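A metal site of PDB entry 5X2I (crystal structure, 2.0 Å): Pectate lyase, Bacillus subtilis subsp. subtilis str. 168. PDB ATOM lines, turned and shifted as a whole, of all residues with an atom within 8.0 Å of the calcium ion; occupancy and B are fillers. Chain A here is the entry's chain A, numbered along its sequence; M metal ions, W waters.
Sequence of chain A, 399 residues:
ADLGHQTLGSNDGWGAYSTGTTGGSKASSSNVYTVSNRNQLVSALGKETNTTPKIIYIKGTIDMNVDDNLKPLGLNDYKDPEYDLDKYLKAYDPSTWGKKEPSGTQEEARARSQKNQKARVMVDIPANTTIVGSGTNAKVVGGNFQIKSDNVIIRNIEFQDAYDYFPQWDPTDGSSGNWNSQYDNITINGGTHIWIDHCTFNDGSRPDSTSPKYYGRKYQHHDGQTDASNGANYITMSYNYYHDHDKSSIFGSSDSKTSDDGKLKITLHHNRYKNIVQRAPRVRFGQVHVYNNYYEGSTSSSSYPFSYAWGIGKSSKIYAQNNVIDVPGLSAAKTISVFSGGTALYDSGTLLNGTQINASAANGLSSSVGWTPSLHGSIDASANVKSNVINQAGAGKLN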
ATOM      1  N   ASN A 144      18.861  21.405  22.115  1.00  0.00           N
ATOM      2  CA  ASN A 144      19.037  22.690  21.401  1.00  0.00           C
ATOM      3  C   ASN A 144      20.566  22.791  21.202  1.00  0.00           C
ATOM      4  O   ASN A 144      21.308  22.966  22.178  1.00  0.00           O
ATOM      5  CB  ASN A 144      18.514  23.800  22.302  1.00  0.00           C
ATOM      6  CG  ASN A 144      18.524  25.204  21.690  1.00  0.00           C
ATOM      7  OD1 ASN A 144      17.797  26.045  22.177  1.00  0.00           O
ATOM      8  ND2 ASN A 144      19.324  25.485  20.643  1.00  0.00           N
ATOM      9  N   SER A 181       8.743  29.961  24.753  1.00  0.00           N
ATOM     10  CA  SER A 181       9.651  28.979  25.230  1.00  0.00           C
ATOM     11  C   SER A 181      11.059  29.304  24.717  1.00  0.00           C
ATOM     12  O   SER A 181      11.229  30.140  23.868  1.00  0.00           O
ATOM     13  CB  SER A 181       9.131  27.588  24.863  1.00  0.00           C
ATOM     14  OG  SER A 181       8.126  27.161  25.812  1.00  0.00           O
ATOM     15  N   GLN A 182      12.086  28.646  25.221  1.00  0.00           N
ATOM     16  CA  GLN A 182      13.484  29.062  25.012  1.00  0.00           C
ATOM     17  C   GLN A 182      14.225  28.254  23.968  1.00  0.00           C
ATOM     18  O   GLN A 182      15.282  28.673  23.466  1.00  0.00           O
ATOM     19  CB  GLN A 182      14.289  28.886  26.342  1.00  0.00           C
ATOM     20  CG  GLN A 182      14.194  30.038  27.302  1.00  0.00           C
ATOM     21  CD  GLN A 182      15.433  30.915  27.289  1.00  0.00           C
ATOM     22  OE1 GLN A 182      16.529  30.500  27.690  1.00  0.00           O
ATOM     23  NE2 GLN A 182      15.271  32.142  26.797  1.00  0.00           N
ATOM     24  N   TYR A 183      13.765  27.031  23.727  1.00  0.00           N
ATOM     25  CA  TYR A 183      14.560  26.034  23.001  1.00  0.00           C
ATOM     26  C   TYR A 183      14.203  25.904  21.527  1.00  0.00           C
ATOM     27  O   TYR A 183      13.074  25.575  21.201  1.00  0.00           O
ATOM     28  CB  TYR A 183      14.579  24.656  23.679  1.00  0.00           C
ATOM     29  CG  TYR A 183      14.883  24.783  25.161  1.00  0.00           C
ATOM     30  CD1 TYR A 183      16.013  25.461  25.616  1.00  0.00           C
ATOM     31  CD2 TYR A 183      13.955  24.367  26.123  1.00  0.00           C
ATOM     32  CE1 TYR A 183      16.250  25.694  26.953  1.00  0.00           C
ATOM     33  CE2 TYR A 183      14.225  24.538  27.465  1.00  0.00           C
ATOM     34  CZ  TYR A 183      15.343  25.260  27.891  1.00  0.00           C
ATOM     35  OH  TYR A 183      15.586  25.453  29.240  1.00  0.00           O
ATOM     36  N   ASP A 184      15.215  26.093  20.681  1.00  0.00           N
ATOM     37  CA  ASP A 184      15.205  25.764  19.243  1.00  0.00           C
ATOM     38  C   ASP A 184      15.850  24.406  19.071  1.00  0.00           C
ATOM     39  O   ASP A 184      16.473  23.906  19.996  1.00  0.00           O
ATOM     40  CB  ASP A 184      16.039  26.780  18.472  1.00  0.00           C
ATOM     41  CG  ASP A 184      15.599  28.234  18.735  1.00  0.00           C
ATOM     42  OD1 ASP A 184      14.374  28.447  18.825  1.00  0.00           O
ATOM     43  OD2 ASP A 184      16.436  29.148  18.839  1.00  0.00           O
ATOM     44  N   ASN A 185      15.730  23.802  17.895  1.00  0.00           N
ATOM     45  CA  ASN A 185      16.536  22.632  17.622  1.00  0.00           C
ATOM     46  C   ASN A 185      17.984  23.070  17.392  1.00  0.00           C
ATOM     47  O   ASN A 185      18.935  22.489  17.975  1.00  0.00           O
ATOM     48  CB  ASN A 185      16.058  21.878  16.377  1.00  0.00           C
ATOM     49  CG  ASN A 185      14.583  21.536  16.428  1.00  0.00           C
ATOM     50  OD1 ASN A 185      13.772  22.095  15.683  1.00  0.00           O
ATOM     51  ND2 ASN A 185      14.227  20.626  17.335  1.00  0.00           N
ATOM     52  N   ILE A 186      18.150  24.156  16.629  1.00  0.00           N
ATOM     53  CA  ILE A 186      19.446  24.805  16.473  1.00  0.00           C
ATOM     54  C   ILE A 186      19.337  26.296  16.610  1.00  0.00           C
ATOM     55  O   ILE A 186      18.501  26.922  15.932  1.00  0.00           O
ATOM     56  CB  ILE A 186      20.105  24.499  15.095  1.00  0.00           C
ATOM     57  CG1 ILE A 186      20.232  22.973  14.850  1.00  0.00           C
ATOM     58  CG2 ILE A 186      21.439  25.226  14.930  1.00  0.00           C
ATOM     59  CD1 ILE A 186      20.701  22.622  13.439  1.00  0.00           C
ATOM     60  N   THR A 187      20.199  26.885  17.444  1.00  0.00           N
ATOM     61  CA  THR A 187      20.244  28.366  17.616  1.00  0.00           C
ATOM     62  C   THR A 187      21.608  28.809  17.213  1.00  0.00           C
ATOM     63  O   THR A 187      22.568  28.356  17.809  1.00  0.00           O
ATOM     64  CB  THR A 187      20.065  28.780  19.092  1.00  0.00           C
ATOM     65  OG1 THR A 187      18.903  28.129  19.605  1.00  0.00           O
ATOM     66  CG2 THR A 187      19.881  30.265  19.193  1.00  0.00           C
ATOM     67  N   ILE A 188      21.699  29.641  16.194  1.00  0.00           N
ATOM     68  CA  ILE A 188      22.975  30.225  15.792  1.00  0.00           C
ATOM     69  C   ILE A 188      23.062  31.628  16.469  1.00  0.00           C
ATOM     70  O   ILE A 188      22.517  32.614  15.965  1.00  0.00           O
ATOM     71  CB  ILE A 188      23.089  30.318  14.269  1.00  0.00           C
ATOM     72  CG1 ILE A 188      22.842  28.947  13.595  1.00  0.00           C
ATOM     73  CG2 ILE A 188      24.449  30.940  13.915  1.00  0.00           C
ATOM     74  CD1 ILE A 188      22.698  29.029  12.080  1.00  0.00           C
ATOM     75  N   HIS A 222       7.359  24.903  22.534  1.00  0.00           N
ATOM     76  CA  HIS A 222       8.402  24.930  21.494  1.00  0.00           C
ATOM     77  C   HIS A 222       8.755  26.332  21.139  1.00  0.00           C
ATOM     78  O   HIS A 222       7.995  27.222  21.461  1.00  0.00           O
ATOM     79  CB  HIS A 222       7.863  24.248  20.248  1.00  0.00           C
ATOM     80  CG  HIS A 222       7.573  22.818  20.443  1.00  0.00           C
ATOM     81  ND1 HIS A 222       6.307  22.294  20.302  1.00  0.00           N
ATOM     82  CD2 HIS A 222       8.356  21.809  20.905  1.00  0.00           C
ATOM     83  CE1 HIS A 222       6.344  20.991  20.550  1.00  0.00           C
ATOM     84  NE2 HIS A 222       7.580  20.678  20.950  1.00  0.00           N
ATOM     85  N   ASP A 223       9.927  26.540  20.518  1.00  0.00           N
ATOM     86  CA  ASP A 223      10.234  27.867  19.970  1.00  0.00           C
ATOM     87  C   ASP A 223      10.619  27.686  18.528  1.00  0.00           C
ATOM     88  O   ASP A 223       9.827  27.119  17.754  1.00  0.00           O
ATOM     89  CB  ASP A 223      11.279  28.591  20.832  1.00  0.00           C
ATOM     90  CG  ASP A 223      11.321  30.101  20.535  1.00  0.00           C
ATOM     91  OD1 ASP A 223      10.231  30.741  20.576  1.00  0.00           O
ATOM     92  OD2 ASP A 223      12.381  30.589  20.175  1.00  0.00           O
ATOM     93  N   GLY A 224      11.845  28.037  18.115  1.00  0.00           N
ATOM     94  CA  GLY A 224      12.217  27.848  16.713  1.00  0.00           C
ATOM     95  C   GLY A 224      12.727  26.466  16.362  1.00  0.00           C
ATOM     96  O   GLY A 224      12.906  25.577  17.216  1.00  0.00           O
ATOM     97  N   GLN A 225      13.040  26.320  15.085  1.00  0.00           N
ATOM     98  CA  GLN A 225      13.703  25.122  14.561  1.00  0.00           C
ATOM     99  C   GLN A 225      15.158  25.462  14.310  1.00  0.00           C
ATOM    100  O   GLN A 225      16.037  24.905  14.981  1.00  0.00           O
ATOM    101  CB  GLN A 225      12.987  24.613  13.311  1.00  0.00           C
ATOM    102  CG  GLN A 225      11.541  24.296  13.651  1.00  0.00           C
ATOM    103  CD  GLN A 225      10.725  23.757  12.483  1.00  0.00           C
ATOM    104  OE1 GLN A 225      10.385  24.489  11.565  1.00  0.00           O
ATOM    105  NE2 GLN A 225      10.395  22.482  12.563  1.00  0.00           N
ATOM    106  N   THR A 226      15.431  26.347  13.358  1.00  0.00           N
ATOM    107  CA  THR A 226      16.791  26.858  13.105  1.00  0.00           C
ATOM    108  C   THR A 226      16.719  28.419  13.139  1.00  0.00           C
ATOM    109  O   THR A 226      16.225  29.070  12.199  1.00  0.00           O
ATOM    110  CB  THR A 226      17.317  26.397  11.699  1.00  0.00           C
ATOM    111  OG1 THR A 226      16.379  26.764  10.679  1.00  0.00           O
ATOM    112  CG2 THR A 226      17.449  24.953  11.666  1.00  0.00           C
ATOM    113  N   ASP A 227      17.159  29.004  14.251  1.00  0.00           N
ATOM    114  CA  ASP A 227      17.097  30.465  14.435  1.00  0.00           C
ATOM    115  C   ASP A 227      18.490  31.044  14.376  1.00  0.00           C
ATOM    116  O   ASP A 227      19.463  30.323  14.514  1.00  0.00           O
ATOM    117  CB  ASP A 227      16.466  30.843  15.769  1.00  0.00           C
ATOM    118  CG  ASP A 227      14.958  30.564  15.815  1.00  0.00           C
ATOM    119  OD1 ASP A 227      14.340  30.327  14.764  1.00  0.00           O
ATOM    120  OD2 ASP A 227      14.388  30.681  16.927  1.00  0.00           O
ATOM    121  N   ALA A 228      18.579  32.337  14.139  1.00  0.00           N
ATOM    122  CA  ALA A 228      19.855  33.057  14.094  1.00  0.00           C
ATOM    123  C   ALA A 228      19.722  34.410  14.740  1.00  0.00           C
ATOM    124  O   ALA A 228      18.809  35.162  14.408  1.00  0.00           O
ATOM    125  CB  ALA A 228      20.370  33.192  12.674  1.00  0.00           C
ATOM    126  N   SER A 229      20.668  34.740  15.619  1.00  0.00           N
ATOM    127  CA  SER A 229      20.594  35.982  16.336  1.00  0.00           C
ATOM    128  C   SER A 229      21.964  36.546  16.607  1.00  0.00           C
ATOM    129  O   SER A 229      22.967  35.875  16.360  1.00  0.00           O
ATOM    130  CB  SER A 229      19.834  35.742  17.631  1.00  0.00           C
ATOM    131  OG  SER A 229      20.582  34.807  18.388  1.00  0.00           O
ATOM    132  N   LYS A 247       6.624  28.021  14.943  1.00  0.00           N
ATOM    133  CA  LYS A 247       7.594  29.066  14.549  1.00  0.00           C
ATOM    134  C   LYS A 247       8.893  28.450  13.993  1.00  0.00           C
ATOM    135  O   LYS A 247       9.702  27.926  14.742  1.00  0.00           O
ATOM    136  CB  LYS A 247       7.875  30.006  15.750  1.00  0.00           C
ATOM    137  CG  LYS A 247       6.610  30.548  16.389  1.00  0.00           C
ATOM    138  CD  LYS A 247       6.817  31.467  17.617  1.00  0.00           C
ATOM    139  CE  LYS A 247       7.146  30.730  18.878  1.00  0.00           C
ATOM    140  NZ  LYS A 247       6.478  31.333  20.083  1.00  0.00           N
ATOM    141  N   SER A 248       9.080  28.459  12.675  1.00  0.00           N
ATOM    142  CA  SER A 248      10.221  27.730  12.077  1.00  0.00           C
ATOM    143  C   SER A 248      11.599  28.407  12.202  1.00  0.00           C
ATOM    144  O   SER A 248      12.494  27.841  12.780  1.00  0.00           O
ATOM    145  CB  SER A 248       9.974  27.358  10.620  1.00  0.00           C
ATOM    146  OG  SER A 248      11.164  26.812  10.063  1.00  0.00           O
ATOM    147  N   SER A 249      11.774  29.602  11.657  1.00  0.00           N
ATOM    148  CA  SER A 249      13.099  30.158  11.382  1.00  0.00           C
ATOM    149  C   SER A 249      13.096  31.668  11.543  1.00  0.00           C
ATOM    150  O   SER A 249      12.545  32.359  10.679  1.00  0.00           O
ATOM    151  CB  SER A 249      13.531  29.817   9.915  1.00  0.00           C
ATOM    152  OG  SER A 249      13.719  28.406   9.777  1.00  0.00           O
ATOM    153  N   ILE A 250      13.624  32.166  12.676  1.00  0.00           N
ATOM    154  CA  ILE A 250      13.639  33.589  12.984  1.00  0.00           C
ATOM    155  C   ILE A 250      15.062  34.070  12.896  1.00  0.00           C
ATOM    156  O   ILE A 250      15.922  33.509  13.590  1.00  0.00           O
ATOM    157  CB  ILE A 250      13.099  33.893  14.408  1.00  0.00           C
ATOM    158  CG1 ILE A 250      11.612  33.462  14.502  1.00  0.00           C
ATOM    159  CG2 ILE A 250      13.205  35.370  14.759  1.00  0.00           C
ATOM    160  CD1 ILE A 250      11.390  31.944  14.636  1.00  0.00           C
ATOM    161  N   SER A 253      16.670  38.707  16.321  1.00  0.00           N
ATOM    162  CA  SER A 253      15.762  38.535  17.452  1.00  0.00           C
ATOM    163  C   SER A 253      15.065  39.819  17.935  1.00  0.00           C
ATOM    164  O   SER A 253      14.129  39.714  18.726  1.00  0.00           O
ATOM    165  CB  SER A 253      16.489  37.935  18.630  1.00  0.00           C
ATOM    166  OG  SER A 253      17.523  38.822  19.049  1.00  0.00           O
HETATM  167 CA    CA M   1      14.721  30.644  19.230  1.00  0.00          CA
HETATM  168  O   HOH W   1      15.519  34.027  19.096  1.00  0.00           O
HETATM  169  O   HOH W   2      15.470  30.787  21.408  1.00  0.00           O
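Three residues have an atom within 4 Å of the calcium ion: Asp 184, Asp 223 and Asp 227.
The backbone carbonyl oxygen (O) of Ile 186 lies within hydrogen-bond range of the backbone NH (N) of Asp 227 (3.0 Å).
OD1 of Asn 144 lies within hydrogen-bond range of N of Asp 184, 3.0 Å away.
The side-chain carboxylate of Asp 184 lies close to the backbone NH of Gly 224 (2.7 Å).
The backbone carbonyl oxygen (O) of Asp 227 is in hydrogen-bond range of the backbone NH (N) of Ile 188 (2.9 Å).
OD2 of Asp 184 sits close to OG1 of Thr 187, 2.8 Å away.
OD1 of Asp 223 is in salt-bridge range of NZ of Lys 247 (3.8 Å).
The backbone carbonyl oxygen (O) of Tyr 183 lies within hydrogen-bond range of the backbone NH (N) of Asp 223, 3.4 Å away.
OD1 of Asp 227 lies within hydrogen-bond range of N of Ile 250 (2.9 Å).
The calcium ion is bound by OD1 of Asp 184 (2.3 Å), water W2 (2.3 Å), OD2 of Asp 184 (2.3 Å), OD2 of Asp 227 (2.3 Å) and OD2 of Asp 223 (2.5 Å).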
